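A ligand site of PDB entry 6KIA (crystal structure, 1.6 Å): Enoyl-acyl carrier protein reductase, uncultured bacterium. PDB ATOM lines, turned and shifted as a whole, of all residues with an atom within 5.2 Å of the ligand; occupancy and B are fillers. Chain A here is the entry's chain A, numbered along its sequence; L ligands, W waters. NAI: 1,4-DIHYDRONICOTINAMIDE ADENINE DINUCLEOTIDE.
Water W1 lies within hydrogen-bond range of an oxygen (O2D) of the ligand (2.5 Å) and the side-chain hydroxyl (OH) of Tyr 260 (3.1 Å). Water W5 bridges an oxygen (O2B) of the ligand (2.7 Å) and the side-chain carboxylate (OE1) of Glu 27 (3.0 Å). Water W4 lies within hydrogen-bond range of an oxygen (O1A) of the ligand, the backbone NH of Phe 29 and the backbone carbonyl oxygen of Glu 27. Water W2 lies within hydrogen-bond range of an oxygen (O1A) of the ligand (2.9 Å), the backbone NH of Asn 294 (2.9 Å), the backbone carbonyl oxygen of Gly 30 (3.0 Å) and the backbone NH of Gly 32 (3.3 Å). Water W3 lies within hydrogen-bond range of O1N of the ligand, N of Ala 34 and N of Tyr 33. Water W7 bridges the backbone NH (N) of Tyr 239 and an oxygen (O3D) of the ligand.
SD of Met 161 lies close to N3A of the ligand. C of Gly 26 touches O3B of the ligand, 3.7 Å away. CD2 of Phe 29 touches O1A of the ligand, at 3.8 Å. Gly 32 touches the ligand (CA to O1N, 3.4 Å). Val 53 touches the ligand. Leu 86 touches the ligand (O to C2A, 3.8 Å). CG1 of Val 208 touches C6A of the ligand, at 3.8 Å. CB of Tyr 239 touches O4D of the ligand, 3.3 Å away. Gly 240 touches the ligand (O to C6N, 3.1 Å). Tyr 241 touches the ligand. Tyr 260 touches the ligand. O of Cys 288 touches C5N of the ligand (3.6 Å). Pro 289 touches the ligand. Glu 290 touches the ligand (CA to O7N, 3.7 Å). CB of Asn 294 touches O2A of the ligand (3.5 Å). Hydrophobic or aromatic side chains that line the ligand: Phe 29, Tyr 33, Val 53, Met 87, Ala 88, Met 161, Ala 162, Val 208, Tyr 239, Tyr 241 and Ile 291. Of the 35 residues printed, 26 come within 4 Å of the ligand. The nearest printed residue that does not touch the ligand is Gly 163 (4.4 Å).
OG1 of Thr 293 is in hydrogen-bond range of N of Ser 295 (3.1 Å). OG of Ser 296 sits at hydrogen-bond distance from N of Thr 293, at 3.1 Å. OE2 of Glu 27 lies within hydrogen-bond range of N of Val 53. The backbone carbonyl oxygen (O) of Tyr 33 is in hydrogen-bond range of the side-chain hydroxyl (OH) of Tyr 239. The backbone carbonyl oxygen of Pro 289 sits at hydrogen-bond distance from the side-chain hydroxyl of Tyr 33 (2.7 Å). The side-chain hydroxyl of Ser 296 sits at hydrogen-bond distance from the backbone carbonyl oxygen of Ile 291, 2.6 Å away. N of Cys 288 lies within hydrogen-bond range of O of Gly 240, 3.0 Å away. The side-chain amide oxygen (OD1) of Asn 294 lies within hydrogen-bond range of the guanidinium group (NH2) of Arg 31.
OG1 of Thr 293 sits at hydrogen-bond distance from O2N of the ligand. The backbone carbonyl oxygen (O) of Thr 160 lies within hydrogen-bond range of an oxygen (O3D) of the ligand (3.0 Å). The side-chain hydroxyl of Thr 160 sits at hydrogen-bond distance from an oxygen (O3B) of the ligand (2.6 Å). An oxygen (O2B) of the ligand is in hydrogen-bond range of the backbone NH (N) of Glu 27. O3B of the ligand sits at hydrogen-bond distance from O of Glu 27, 2.7 Å away. The backbone NH (N) of Tyr 33 lies within hydrogen-bond range of an oxygen (O1N) of the ligand (2.8 Å). The side-chain amino group (NZ) of Lys 266 sits at hydrogen-bond distance from an oxygen (O2D) of the ligand (2.8 Å). OG of Ser 295 lies within hydrogen-bond range of O2N of the ligand, at 2.8 Å. A nitrogen (N1A) of the ligand sits at hydrogen-bond distance from the backbone NH (N) of Ala 88. The backbone carbonyl oxygen of Ala 88 lies within hydrogen-bond range of a nitrogen (N6A) of the ligand (2.9 Å). The backbone NH (N) of Ala 162 lies within hydrogen-bond range of an oxygen (O4B) of the ligand. An oxygen (O7N) of the ligand sits at hydrogen-bond distance from the backbone NH of Ile 291, at 3.1 Å. OG of Ser 296 is in hydrogen-bond range of N7N of the ligand. SD of Met 87 lies within hydrogen-bond range of N6A of the ligand, 3.7 Å away.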
ATOM      1  N   GLY A  26       9.649 -15.356 -10.454  1.00  0.00           N
ATOM      2  CA  GLY A  26       8.357 -15.499  -9.801  1.00  0.00           C
ATOM      3  C   GLY A  26       8.047 -14.171  -9.131  1.00  0.00           C
ATOM      4  O   GLY A  26       8.929 -13.308  -9.046  1.00  0.00           O
ATOM      5  N   GLU A  27       6.823 -14.003  -8.627  1.00  0.00           N
ATOM      6  CA  GLU A  27       6.472 -12.772  -7.919  1.00  0.00           C
ATOM      7  C   GLU A  27       6.533 -12.957  -6.415  1.00  0.00           C
ATOM      8  O   GLU A  27       6.290 -14.052  -5.911  1.00  0.00           O
ATOM      9  CB  GLU A  27       5.082 -12.258  -8.333  1.00  0.00           C
ATOM     10  CG  GLU A  27       5.004 -11.861  -9.811  1.00  0.00           C
ATOM     11  CD  GLU A  27       3.696 -11.175 -10.176  1.00  0.00           C
ATOM     12  OE1 GLU A  27       2.654 -11.491  -9.549  1.00  0.00           O
ATOM     13  OE2 GLU A  27       3.730 -10.280 -11.038  1.00  0.00           O
ATOM     14  N   LEU A  28       6.879 -11.879  -5.719  1.00  0.00           N
ATOM     15  CA  LEU A  28       7.059 -11.888  -4.282  1.00  0.00           C
ATOM     16  C   LEU A  28       5.767 -11.426  -3.604  1.00  0.00           C
ATOM     17  O   LEU A  28       5.258 -10.328  -3.904  1.00  0.00           O
ATOM     18  CB  LEU A  28       8.214 -10.956  -3.890  1.00  0.00           C
ATOM     19  CG  LEU A  28       8.526 -10.933  -2.404  1.00  0.00           C
ATOM     20  CD1 LEU A  28       9.069 -12.312  -1.983  1.00  0.00           C
ATOM     21  CD2 LEU A  28       9.584  -9.844  -2.149  1.00  0.00           C
ATOM     22  N   PHE A  29       5.218 -12.260  -2.714  1.00  0.00           N
ATOM     23  CA  PHE A  29       4.008 -11.905  -1.959  1.00  0.00           C
ATOM     24  C   PHE A  29       4.309 -11.999  -0.485  1.00  0.00           C
ATOM     25  O   PHE A  29       5.201 -12.731  -0.093  1.00  0.00           O
ATOM     26  CB  PHE A  29       2.842 -12.834  -2.279  1.00  0.00           C
ATOM     27  CG  PHE A  29       2.379 -12.744  -3.696  1.00  0.00           C
ATOM     28  CD1 PHE A  29       1.581 -11.697  -4.109  1.00  0.00           C
ATOM     29  CD2 PHE A  29       2.734 -13.709  -4.621  1.00  0.00           C
ATOM     30  CE1 PHE A  29       1.152 -11.605  -5.420  1.00  0.00           C
ATOM     31  CE2 PHE A  29       2.300 -13.624  -5.938  1.00  0.00           C
ATOM     32  CZ  PHE A  29       1.518 -12.570  -6.336  1.00  0.00           C
ATOM     33  N   GLY A  30       3.531 -11.285   0.333  1.00  0.00           N
ATOM     34  CA  GLY A  30       3.631 -11.461   1.764  1.00  0.00           C
ATOM     35  C   GLY A  30       3.378 -12.919   2.113  1.00  0.00           C
ATOM     36  O   GLY A  30       2.516 -13.556   1.491  1.00  0.00           O
ATOM     37  N   ARG A  31       4.162 -13.419   3.062  1.00  0.00           N
ATOM     38  CA  ARG A  31       4.151 -14.809   3.573  1.00  0.00           C
ATOM     39  C   ARG A  31       4.804 -15.793   2.598  1.00  0.00           C
ATOM     40  O   ARG A  31       4.996 -16.972   2.923  1.00  0.00           O
ATOM     41  CB  ARG A  31       2.711 -15.258   3.891  1.00  0.00           C
ATOM     42  CG  ARG A  31       1.981 -14.276   4.792  1.00  0.00           C
ATOM     43  CD  ARG A  31       0.489 -14.495   4.756  1.00  0.00           C
ATOM     44  NE  ARG A  31       0.056 -15.753   5.316  1.00  0.00           N
ATOM     45  CZ  ARG A  31      -0.835 -16.571   4.750  1.00  0.00           C
ATOM     46  NH1 ARG A  31      -1.176 -17.688   5.368  1.00  0.00           N
ATOM     47  NH2 ARG A  31      -1.368 -16.278   3.577  1.00  0.00           N
ATOM     48  N   GLY A  32       5.183 -15.330   1.411  1.00  0.00           N
ATOM     49  CA  GLY A  32       5.781 -16.221   0.439  1.00  0.00           C
ATOM     50  C   GLY A  32       7.147 -16.770   0.861  1.00  0.00           C
ATOM     51  O   GLY A  32       7.938 -16.047   1.472  1.00  0.00           O
ATOM     52  N   TYR A  33       7.437 -18.032   0.517  1.00  0.00           N
ATOM     53  CA  TYR A  33       8.733 -18.624   0.854  1.00  0.00           C
ATOM     54  C   TYR A  33       9.901 -17.759   0.423  1.00  0.00           C
ATOM     55  O   TYR A  33      10.890 -17.655   1.147  1.00  0.00           O
ATOM     56  CB  TYR A  33       8.941 -20.017   0.199  1.00  0.00           C
ATOM     57  CG  TYR A  33       8.833 -21.162   1.162  1.00  0.00           C
ATOM     58  CD1 TYR A  33       9.803 -21.322   2.144  1.00  0.00           C
ATOM     59  CD2 TYR A  33       7.882 -22.162   1.012  1.00  0.00           C
ATOM     60  CE1 TYR A  33       9.763 -22.342   3.034  1.00  0.00           C
ATOM     61  CE2 TYR A  33       7.850 -23.233   1.902  1.00  0.00           C
ATOM     62  CZ  TYR A  33       8.788 -23.310   2.917  1.00  0.00           C
ATOM     63  OH  TYR A  33       8.816 -24.336   3.845  1.00  0.00           O
ATOM     64  N   ALA A  34       9.791 -17.163  -0.768  1.00  0.00           N
ATOM     65  CA  ALA A  34      10.902 -16.432  -1.359  1.00  0.00           C
ATOM     66  C   ALA A  34      11.402 -15.291  -0.478  1.00  0.00           C
ATOM     67  O   ALA A  34      12.553 -14.865  -0.621  1.00  0.00           O
ATOM     68  CB  ALA A  34      10.497 -15.882  -2.747  1.00  0.00           C
ATOM     69  N   VAL A  53       4.354 -11.220 -13.769  1.00  0.00           N
ATOM     70  CA  VAL A  53       3.492 -12.023 -14.625  1.00  0.00           C
ATOM     71  C   VAL A  53       2.577 -11.105 -15.443  1.00  0.00           C
ATOM     72  O   VAL A  53       1.820 -11.559 -16.299  1.00  0.00           O
ATOM     73  CB  VAL A  53       2.643 -13.030 -13.836  1.00  0.00           C
ATOM     74  CG1 VAL A  53       3.551 -14.045 -13.138  1.00  0.00           C
ATOM     75  CG2 VAL A  53       1.741 -12.307 -12.835  1.00  0.00           C
ATOM     76  N   LEU A  86       5.243 -12.379 -17.843  1.00  0.00           N
ATOM     77  CA  LEU A  86       5.720 -13.747 -17.854  1.00  0.00           C
ATOM     78  C   LEU A  86       4.733 -14.657 -17.138  1.00  0.00           C
ATOM     79  O   LEU A  86       5.089 -15.349 -16.173  1.00  0.00           O
ATOM     80  CB  LEU A  86       7.089 -13.856 -17.175  1.00  0.00           C
ATOM     81  CG  LEU A  86       8.357 -13.846 -18.028  1.00  0.00           C
ATOM     82  CD1 LEU A  86       9.555 -14.322 -17.195  1.00  0.00           C
ATOM     83  CD2 LEU A  86       8.203 -14.660 -19.298  1.00  0.00           C
ATOM     84  N   MET A  87       3.490 -14.629 -17.603  1.00  0.00           N
ATOM     85  CA  MET A  87       2.463 -15.513 -17.054  1.00  0.00           C
ATOM     86  C   MET A  87       2.597 -16.931 -17.592  1.00  0.00           C
ATOM     87  O   MET A  87       2.523 -17.145 -18.790  1.00  0.00           O
ATOM     88  CB  MET A  87       1.074 -14.990 -17.411  1.00  0.00           C
ATOM     89  CG  MET A  87      -0.001 -15.795 -16.765  1.00  0.00           C
ATOM     90  SD  MET A  87      -0.286 -15.276 -15.089  1.00  0.00           S
ATOM     91  CE  MET A  87      -1.402 -13.907 -15.409  1.00  0.00           C
ATOM     92  N   ALA A  88       2.801 -17.903 -16.704  1.00  0.00           N
ATOM     93  CA  ALA A  88       2.895 -19.293 -17.143  1.00  0.00           C
ATOM     94  C   ALA A  88       1.522 -19.942 -17.204  1.00  0.00           C
ATOM     95  O   ALA A  88       0.545 -19.382 -16.720  1.00  0.00           O
ATOM     96  CB  ALA A  88       3.797 -20.081 -16.261  1.00  0.00           C
ATOM     97  N   GLY A  89       1.467 -21.124 -17.817  1.00  0.00           N
ATOM     98  CA  GLY A  89       0.210 -21.833 -17.981  1.00  0.00           C
ATOM     99  C   GLY A  89      -0.418 -21.461 -19.305  1.00  0.00           C
ATOM    100  O   GLY A  89      -0.022 -20.495 -19.962  1.00  0.00           O
ATOM    101  N   THR A 160      10.320 -19.740  -8.299  1.00  0.00           N
ATOM    102  CA  THR A 160       9.328 -19.888  -7.227  1.00  0.00           C
ATOM    103  C   THR A 160       7.981 -20.339  -7.764  1.00  0.00           C
ATOM    104  O   THR A 160       7.037 -20.518  -6.996  1.00  0.00           O
ATOM    105  CB  THR A 160       9.070 -18.569  -6.452  1.00  0.00           C
ATOM    106  OG1 THR A 160       8.438 -17.633  -7.333  1.00  0.00           O
ATOM    107  CG2 THR A 160      10.370 -17.968  -5.897  1.00  0.00           C
ATOM    108  N   MET A 161       7.855 -20.465  -9.089  1.00  0.00           N
ATOM    109  CA  MET A 161       6.539 -20.583  -9.704  1.00  0.00           C
ATOM    110  C   MET A 161       5.859 -21.900  -9.414  1.00  0.00           C
ATOM    111  O   MET A 161       6.452 -22.959  -9.590  1.00  0.00           O
ATOM    112  CB  MET A 161       6.633 -20.413 -11.223  1.00  0.00           C
ATOM    113  CG  MET A 161       7.210 -19.089 -11.645  1.00  0.00           C
ATOM    114  SD  MET A 161       7.334 -18.919 -13.420  1.00  0.00           S
ATOM    115  CE  MET A 161       7.802 -17.191 -13.579  1.00  0.00           C
ATOM    116  N   ALA A 162       4.606 -21.810  -9.002  1.00  0.00           N
ATOM    117  CA  ALA A 162       3.720 -22.955  -8.836  1.00  0.00           C
ATOM    118  C   ALA A 162       2.294 -22.458  -9.020  1.00  0.00           C
ATOM    119  O   ALA A 162       1.969 -21.371  -8.556  1.00  0.00           O
ATOM    120  CB  ALA A 162       3.908 -23.614  -7.448  1.00  0.00           C
ATOM    121  N   GLY A 163       1.450 -23.253  -9.647  1.00  0.00           N
ATOM    122  CA  GLY A 163       0.058 -22.867  -9.831  1.00  0.00           C
ATOM    123  C   GLY A 163      -0.540 -23.515 -11.057  1.00  0.00           C
ATOM    124  O   GLY A 163      -0.110 -24.598 -11.437  1.00  0.00           O
ATOM    125  N   GLY A 164      -1.533 -22.867 -11.666  1.00  0.00           N
ATOM    126  CA  GLY A 164      -2.146 -23.380 -12.881  1.00  0.00           C
ATOM    127  C   GLY A 164      -3.608 -23.709 -12.682  1.00  0.00           C
ATOM    128  O   GLY A 164      -4.219 -24.362 -13.523  1.00  0.00           O
ATOM    129  N   VAL A 208       3.181 -24.801 -15.269  1.00  0.00           N
ATOM    130  CA  VAL A 208       3.502 -23.700 -14.345  1.00  0.00           C
ATOM    131  C   VAL A 208       4.529 -24.076 -13.278  1.00  0.00           C
ATOM    132  O   VAL A 208       5.468 -23.329 -13.005  1.00  0.00           O
ATOM    133  CB  VAL A 208       2.222 -23.190 -13.613  1.00  0.00           C
ATOM    134  CG1 VAL A 208       2.576 -22.036 -12.671  1.00  0.00           C
ATOM    135  CG2 VAL A 208       1.122 -22.769 -14.641  1.00  0.00           C
ATOM    136  N   TYR A 239      11.812 -23.989  -5.263  1.00  0.00           N
ATOM    137  CA  TYR A 239      11.139 -24.455  -4.056  1.00  0.00           C
ATOM    138  C   TYR A 239      10.325 -25.688  -4.397  1.00  0.00           C
ATOM    139  O   TYR A 239       9.402 -25.615  -5.202  1.00  0.00           O
ATOM    140  CB  TYR A 239      10.239 -23.370  -3.463  1.00  0.00           C
ATOM    141  CG  TYR A 239      10.992 -22.209  -2.826  1.00  0.00           C
ATOM    142  CD1 TYR A 239      11.360 -22.261  -1.482  1.00  0.00           C
ATOM    143  CD2 TYR A 239      11.327 -21.077  -3.575  1.00  0.00           C
ATOM    144  CE1 TYR A 239      12.044 -21.203  -0.898  1.00  0.00           C
ATOM    145  CE2 TYR A 239      12.021 -20.039  -2.991  1.00  0.00           C
ATOM    146  CZ  TYR A 239      12.362 -20.097  -1.670  1.00  0.00           C
ATOM    147  OH  TYR A 239      13.056 -19.069  -1.076  1.00  0.00           O
ATOM    148  N   GLY A 240      10.679 -26.822  -3.808  1.00  0.00           N
ATOM    149  CA  GLY A 240       9.932 -28.032  -4.075  1.00  0.00           C
ATOM    150  C   GLY A 240       9.077 -28.363  -2.882  1.00  0.00           C
ATOM    151  O   GLY A 240       9.325 -27.861  -1.786  1.00  0.00           O
ATOM    152  N   TYR A 241       8.059 -29.195  -3.103  1.00  0.00           N
ATOM    153  CA  TYR A 241       7.416 -29.862  -1.961  1.00  0.00           C
ATOM    154  C   TYR A 241       7.347 -31.350  -2.286  1.00  0.00           C
ATOM    155  O   TYR A 241       6.915 -31.723  -3.373  1.00  0.00           O
ATOM    156  CB  TYR A 241       6.001 -29.341  -1.676  1.00  0.00           C
ATOM    157  CG  TYR A 241       5.400 -30.102  -0.509  1.00  0.00           C
ATOM    158  CD1 TYR A 241       5.907 -29.925   0.777  1.00  0.00           C
ATOM    159  CD2 TYR A 241       4.355 -31.005  -0.697  1.00  0.00           C
ATOM    160  CE1 TYR A 241       5.397 -30.634   1.850  1.00  0.00           C
ATOM    161  CE2 TYR A 241       3.833 -31.710   0.381  1.00  0.00           C
ATOM    162  CZ  TYR A 241       4.351 -31.518   1.641  1.00  0.00           C
ATOM    163  OH  TYR A 241       3.845 -32.215   2.734  1.00  0.00           O
ATOM    164  N   TYR A 260      -1.677 -34.126  -2.131  1.00  0.00           N
ATOM    165  CA  TYR A 260      -1.008 -32.977  -2.744  1.00  0.00           C
ATOM    166  C   TYR A 260      -1.084 -33.043  -4.258  1.00  0.00           C
ATOM    167  O   TYR A 260      -0.308 -33.747  -4.901  1.00  0.00           O
ATOM    168  CB  TYR A 260       0.433 -32.933  -2.256  1.00  0.00           C
ATOM    169  CG  TYR A 260       1.195 -31.733  -2.710  1.00  0.00           C
ATOM    170  CD1 TYR A 260       0.986 -30.490  -2.138  1.00  0.00           C
ATOM    171  CD2 TYR A 260       2.141 -31.851  -3.719  1.00  0.00           C
ATOM    172  CE1 TYR A 260       1.700 -29.371  -2.567  1.00  0.00           C
ATOM    173  CE2 TYR A 260       2.861 -30.738  -4.145  1.00  0.00           C
ATOM    174  CZ  TYR A 260       2.632 -29.514  -3.569  1.00  0.00           C
ATOM    175  OH  TYR A 260       3.352 -28.425  -4.018  1.00  0.00           O
ATOM    176  N   LYS A 266       5.683 -31.520  -9.091  1.00  0.00           N
ATOM    177  CA  LYS A 266       6.884 -31.316  -8.269  1.00  0.00           C
ATOM    178  C   LYS A 266       7.925 -32.420  -8.559  1.00  0.00           C
ATOM    179  O   LYS A 266       9.134 -32.176  -8.459  1.00  0.00           O
ATOM    180  CB  LYS A 266       6.547 -31.299  -6.779  1.00  0.00           C
ATOM    181  CG  LYS A 266       5.795 -30.009  -6.325  1.00  0.00           C
ATOM    182  CD  LYS A 266       6.683 -28.773  -6.561  1.00  0.00           C
ATOM    183  CE  LYS A 266       6.059 -27.529  -5.916  1.00  0.00           C
ATOM    184  NZ  LYS A 266       6.820 -26.261  -6.161  1.00  0.00           N
ATOM    185  N   CYS A 288      10.962 -28.168   0.661  1.00  0.00           N
ATOM    186  CA  CYS A 288      10.785 -27.396   1.906  1.00  0.00           C
ATOM    187  C   CYS A 288       9.566 -27.818   2.699  1.00  0.00           C
ATOM    188  O   CYS A 288       8.656 -28.444   2.150  1.00  0.00           O
ATOM    189  CB  CYS A 288      10.710 -25.902   1.577  1.00  0.00           C
ATOM    190  SG  CYS A 288      12.284 -25.197   0.956  1.00  0.00           S
ATOM    191  N   PRO A 289       9.499 -27.444   3.990  1.00  0.00           N
ATOM    192  CA  PRO A 289       8.337 -27.861   4.803  1.00  0.00           C
ATOM    193  C   PRO A 289       6.999 -27.248   4.440  1.00  0.00           C
ATOM    194  O   PRO A 289       6.896 -26.208   3.803  1.00  0.00           O
ATOM    195  CB  PRO A 289       8.713 -27.373   6.206  1.00  0.00           C
ATOM    196  CG  PRO A 289      10.172 -27.314   6.211  1.00  0.00           C
ATOM    197  CD  PRO A 289      10.535 -26.814   4.826  1.00  0.00           C
ATOM    198  N   GLU A 290       5.932 -27.913   4.906  1.00  0.00           N
ATOM    199  CA  GLU A 290       4.584 -27.380   4.876  1.00  0.00           C
ATOM    200  C   GLU A 290       4.509 -26.094   5.703  1.00  0.00           C
ATOM    201  O   GLU A 290       4.902 -26.082   6.891  1.00  0.00           O
ATOM    202  CB  GLU A 290       3.604 -28.401   5.477  1.00  0.00           C
ATOM    203  CG  GLU A 290       3.641 -29.801   4.857  1.00  0.00           C
ATOM    204  CD  GLU A 290       4.705 -30.726   5.471  1.00  0.00           C
ATOM    205  OE1 GLU A 290       5.525 -30.299   6.327  1.00  0.00           O
ATOM    206  OE2 GLU A 290       4.723 -31.916   5.099  1.00  0.00           O
ATOM    207  N   ILE A 291       4.014 -25.022   5.087  1.00  0.00           N
ATOM    208  CA  ILE A 291       3.745 -23.794   5.805  1.00  0.00           C
ATOM    209  C   ILE A 291       2.452 -23.182   5.292  1.00  0.00           C
ATOM    210  O   ILE A 291       1.834 -23.714   4.371  1.00  0.00           O
ATOM    211  CB  ILE A 291       4.903 -22.771   5.690  1.00  0.00           C
ATOM    212  CG1 ILE A 291       5.204 -22.447   4.231  1.00  0.00           C
ATOM    213  CG2 ILE A 291       6.181 -23.286   6.373  1.00  0.00           C
ATOM    214  CD1 ILE A 291       6.131 -21.261   4.140  1.00  0.00           C
ATOM    215  N   ARG A 292       1.999 -22.086   5.910  1.00  0.00           N
ATOM    216  CA  ARG A 292       0.836 -21.397   5.382  1.00  0.00           C
ATOM    217  C   ARG A 292       1.244 -20.125   4.623  1.00  0.00           C
ATOM    218  O   ARG A 292       1.832 -19.196   5.190  1.00  0.00           O
ATOM    219  CB  ARG A 292      -0.150 -21.070   6.503  1.00  0.00           C
ATOM    220  CG  ARG A 292      -0.759 -22.357   7.059  1.00  0.00           C
ATOM    221  CD  ARG A 292      -1.894 -22.092   8.026  1.00  0.00           C
ATOM    222  NE  ARG A 292      -3.176 -21.866   7.352  1.00  0.00           N
ATOM    223  CZ  ARG A 292      -3.770 -20.683   7.255  1.00  0.00           C
ATOM    224  NH1 ARG A 292      -3.209 -19.605   7.790  1.00  0.00           N
ATOM    225  NH2 ARG A 292      -4.937 -20.579   6.614  1.00  0.00           N
ATOM    226  N   THR A 293       0.972 -20.149   3.327  1.00  0.00           N
ATOM    227  CA  THR A 293       1.201 -19.045   2.404  1.00  0.00           C
ATOM    228  C   THR A 293      -0.057 -18.830   1.573  1.00  0.00           C
ATOM    229  O   THR A 293      -1.047 -19.546   1.722  1.00  0.00           O
ATOM    230  CB  THR A 293       2.347 -19.334   1.423  1.00  0.00           C
ATOM    231  OG1 THR A 293       1.915 -20.388   0.562  1.00  0.00           O
ATOM    232  CG2 THR A 293       3.634 -19.719   2.122  1.00  0.00           C
ATOM    233  N   ASN A 294      -0.013 -17.860   0.654  1.00  0.00           N
ATOM    234  CA  ASN A 294      -1.110 -17.693  -0.293  1.00  0.00           C
ATOM    235  C   ASN A 294      -1.401 -18.974  -1.088  1.00  0.00           C
ATOM    236  O   ASN A 294      -2.571 -19.271  -1.376  1.00  0.00           O
ATOM    237  CB  ASN A 294      -0.805 -16.559  -1.290  1.00  0.00           C
ATOM    238  CG  ASN A 294      -0.857 -15.190  -0.640  1.00  0.00           C
ATOM    239  OD1 ASN A 294      -1.077 -15.052   0.576  1.00  0.00           O
ATOM    240  ND2 ASN A 294      -0.643 -14.154  -1.441  1.00  0.00           N
ATOM    241  N   SER A 295      -0.371 -19.756  -1.414  1.00  0.00           N
ATOM    242  CA  SER A 295      -0.617 -20.927  -2.265  1.00  0.00           C
ATOM    243  C   SER A 295      -1.050 -22.167  -1.474  1.00  0.00           C
ATOM    244  O   SER A 295      -1.627 -23.096  -2.032  1.00  0.00           O
ATOM    245  CB  SER A 295       0.648 -21.266  -3.078  1.00  0.00           C
ATOM    246  OG  SER A 295       1.558 -22.058  -2.296  1.00  0.00           O
ATOM    247  N   SER A 296      -0.830 -22.190  -0.170  1.00  0.00           N
ATOM    248  CA  SER A 296      -1.185 -23.385   0.580  1.00  0.00           C
ATOM    249  C   SER A 296      -2.340 -23.192   1.558  1.00  0.00           C
ATOM    250  O   SER A 296      -2.753 -24.151   2.204  1.00  0.00           O
ATOM    251  CB  SER A 296       0.049 -23.940   1.307  1.00  0.00           C
ATOM    252  OG  SER A 296       0.518 -23.025   2.279  1.00  0.00           O
ATOM    253  N   VAL A 302      -2.772 -28.954   5.980  1.00  0.00           N
ATOM    254  CA  VAL A 302      -1.355 -28.919   5.624  1.00  0.00           C
ATOM    255  C   VAL A 302      -0.513 -28.447   6.832  1.00  0.00           C
ATOM    256  O   VAL A 302       0.604 -28.940   7.091  1.00  0.00           O
ATOM    257  CB  VAL A 302      -1.114 -28.021   4.370  1.00  0.00           C
ATOM    258  CG1 VAL A 302      -1.341 -26.531   4.661  1.00  0.00           C
ATOM    259  CG2 VAL A 302       0.310 -28.267   3.770  1.00  0.00           C
HETATM  260  PA  NAI L   1       3.119 -17.715  -3.081  1.00  0.00           P
HETATM  261  O1A NAI L   1       3.701 -16.559  -2.329  1.00  0.00           O
HETATM  262  O2A NAI L   1       1.667 -17.599  -3.505  1.00  0.00           O
HETATM  263  O5B NAI L   1       4.064 -17.988  -4.333  1.00  0.00           O
HETATM  264  C5B NAI L   1       3.521 -18.511  -5.523  1.00  0.00           C
HETATM  265  C4B NAI L   1       4.607 -18.170  -6.597  1.00  0.00           C
HETATM  266  O4B NAI L   1       4.113 -18.849  -7.899  1.00  0.00           O
HETATM  267  C3B NAI L   1       4.689 -16.906  -6.834  1.00  0.00           C
HETATM  268  O3B NAI L   1       6.101 -16.472  -7.047  1.00  0.00           O
HETATM  269  C2B NAI L   1       3.809 -16.669  -8.207  1.00  0.00           C
HETATM  270  O2B NAI L   1       4.202 -15.387  -8.830  1.00  0.00           O
HETATM  271  C1B NAI L   1       4.079 -17.706  -8.921  1.00  0.00           C
HETATM  272  N9A NAI L   1       2.935 -18.084  -9.775  1.00  0.00           N
HETATM  273  C8A NAI L   1       1.685 -18.545  -9.551  1.00  0.00           C
HETATM  274  N7A NAI L   1       1.092 -18.704 -10.726  1.00  0.00           N
HETATM  275  C5A NAI L   1       1.969 -18.350 -11.693  1.00  0.00           C
HETATM  276  C6A NAI L   1       1.774 -18.344 -13.064  1.00  0.00           C
HETATM  277  N6A NAI L   1       0.673 -18.694 -13.914  1.00  0.00           N
HETATM  278  N1A NAI L   1       2.791 -17.942 -13.852  1.00  0.00           N
HETATM  279  C2A NAI L   1       3.973 -17.539 -13.289  1.00  0.00           C
HETATM  280  N3A NAI L   1       4.169 -17.545 -11.918  1.00  0.00           N
HETATM  281  C4A NAI L   1       3.125 -17.959 -11.130  1.00  0.00           C
HETATM  282  O3  NAI L   1       3.201 -19.112  -2.195  1.00  0.00           O
HETATM  283  PN  NAI L   1       4.486 -20.027  -1.840  1.00  0.00           P
HETATM  284  O1N NAI L   1       5.532 -19.209  -1.138  1.00  0.00           O
HETATM  285  O2N NAI L   1       3.893 -21.134  -0.979  1.00  0.00           O
HETATM  286  O5D NAI L   1       5.047 -20.608  -3.216  1.00  0.00           O
HETATM  287  C5D NAI L   1       6.397 -20.421  -3.609  1.00  0.00           C
HETATM  288  C4D NAI L   1       7.000 -21.805  -3.897  1.00  0.00           C
HETATM  289  O4D NAI L   1       7.116 -22.461  -2.762  1.00  0.00           O
HETATM  290  C3D NAI L   1       6.048 -22.637  -4.754  1.00  0.00           C
HETATM  291  O3D NAI L   1       6.699 -23.254  -5.821  1.00  0.00           O
HETATM  292  C2D NAI L   1       5.600 -23.718  -3.744  1.00  0.00           C
HETATM  293  O2D NAI L   1       5.070 -24.876  -4.483  1.00  0.00           O
HETATM  294  C1D NAI L   1       6.664 -23.952  -3.033  1.00  0.00           C
HETATM  295  N1N NAI L   1       6.391 -24.611  -1.755  1.00  0.00           N
HETATM  296  C2N NAI L   1       5.351 -24.212  -0.942  1.00  0.00           C
HETATM  297  C3N NAI L   1       5.089 -24.908   0.251  1.00  0.00           C
HETATM  298  C7N NAI L   1       3.970 -24.464   1.190  1.00  0.00           C
HETATM  299  O7N NAI L   1       3.531 -25.234   2.045  1.00  0.00           O
HETATM  300  N7N NAI L   1       3.440 -23.155   1.072  1.00  0.00           N
HETATM  301  C4N NAI L   1       5.869 -25.982   0.640  1.00  0.00           C
HETATM  302  C5N NAI L   1       6.956 -26.345  -0.163  1.00  0.00           C
HETATM  303  C6N NAI L   1       7.200 -25.652  -1.357  1.00  0.00           C
HETATM  304  O   HOH W   1       2.707 -25.382  -3.800  1.00  0.00           O
HETATM  305  O   HOH W   2       2.252 -16.149   0.101  1.00  0.00           O
HETATM  306  O   HOH W   3       7.383 -17.338  -2.502  1.00  0.00           O
HETATM  307  O   HOH W   4       5.840 -15.059  -3.139  1.00  0.00           O
HETATM  308  O   HOH W   5       1.907 -14.383  -9.774  1.00  0.00           O
HETATM  309  O   HOH W   6       2.514 -27.368   0.735  1.00  0.00           O
HETATM  310  O   HOH W   7       9.767 -23.249  -7.155  1.00  0.00           O
HETATM  311  O   HOH W   8       0.066 -15.965  -4.599  1.00  0.00           O
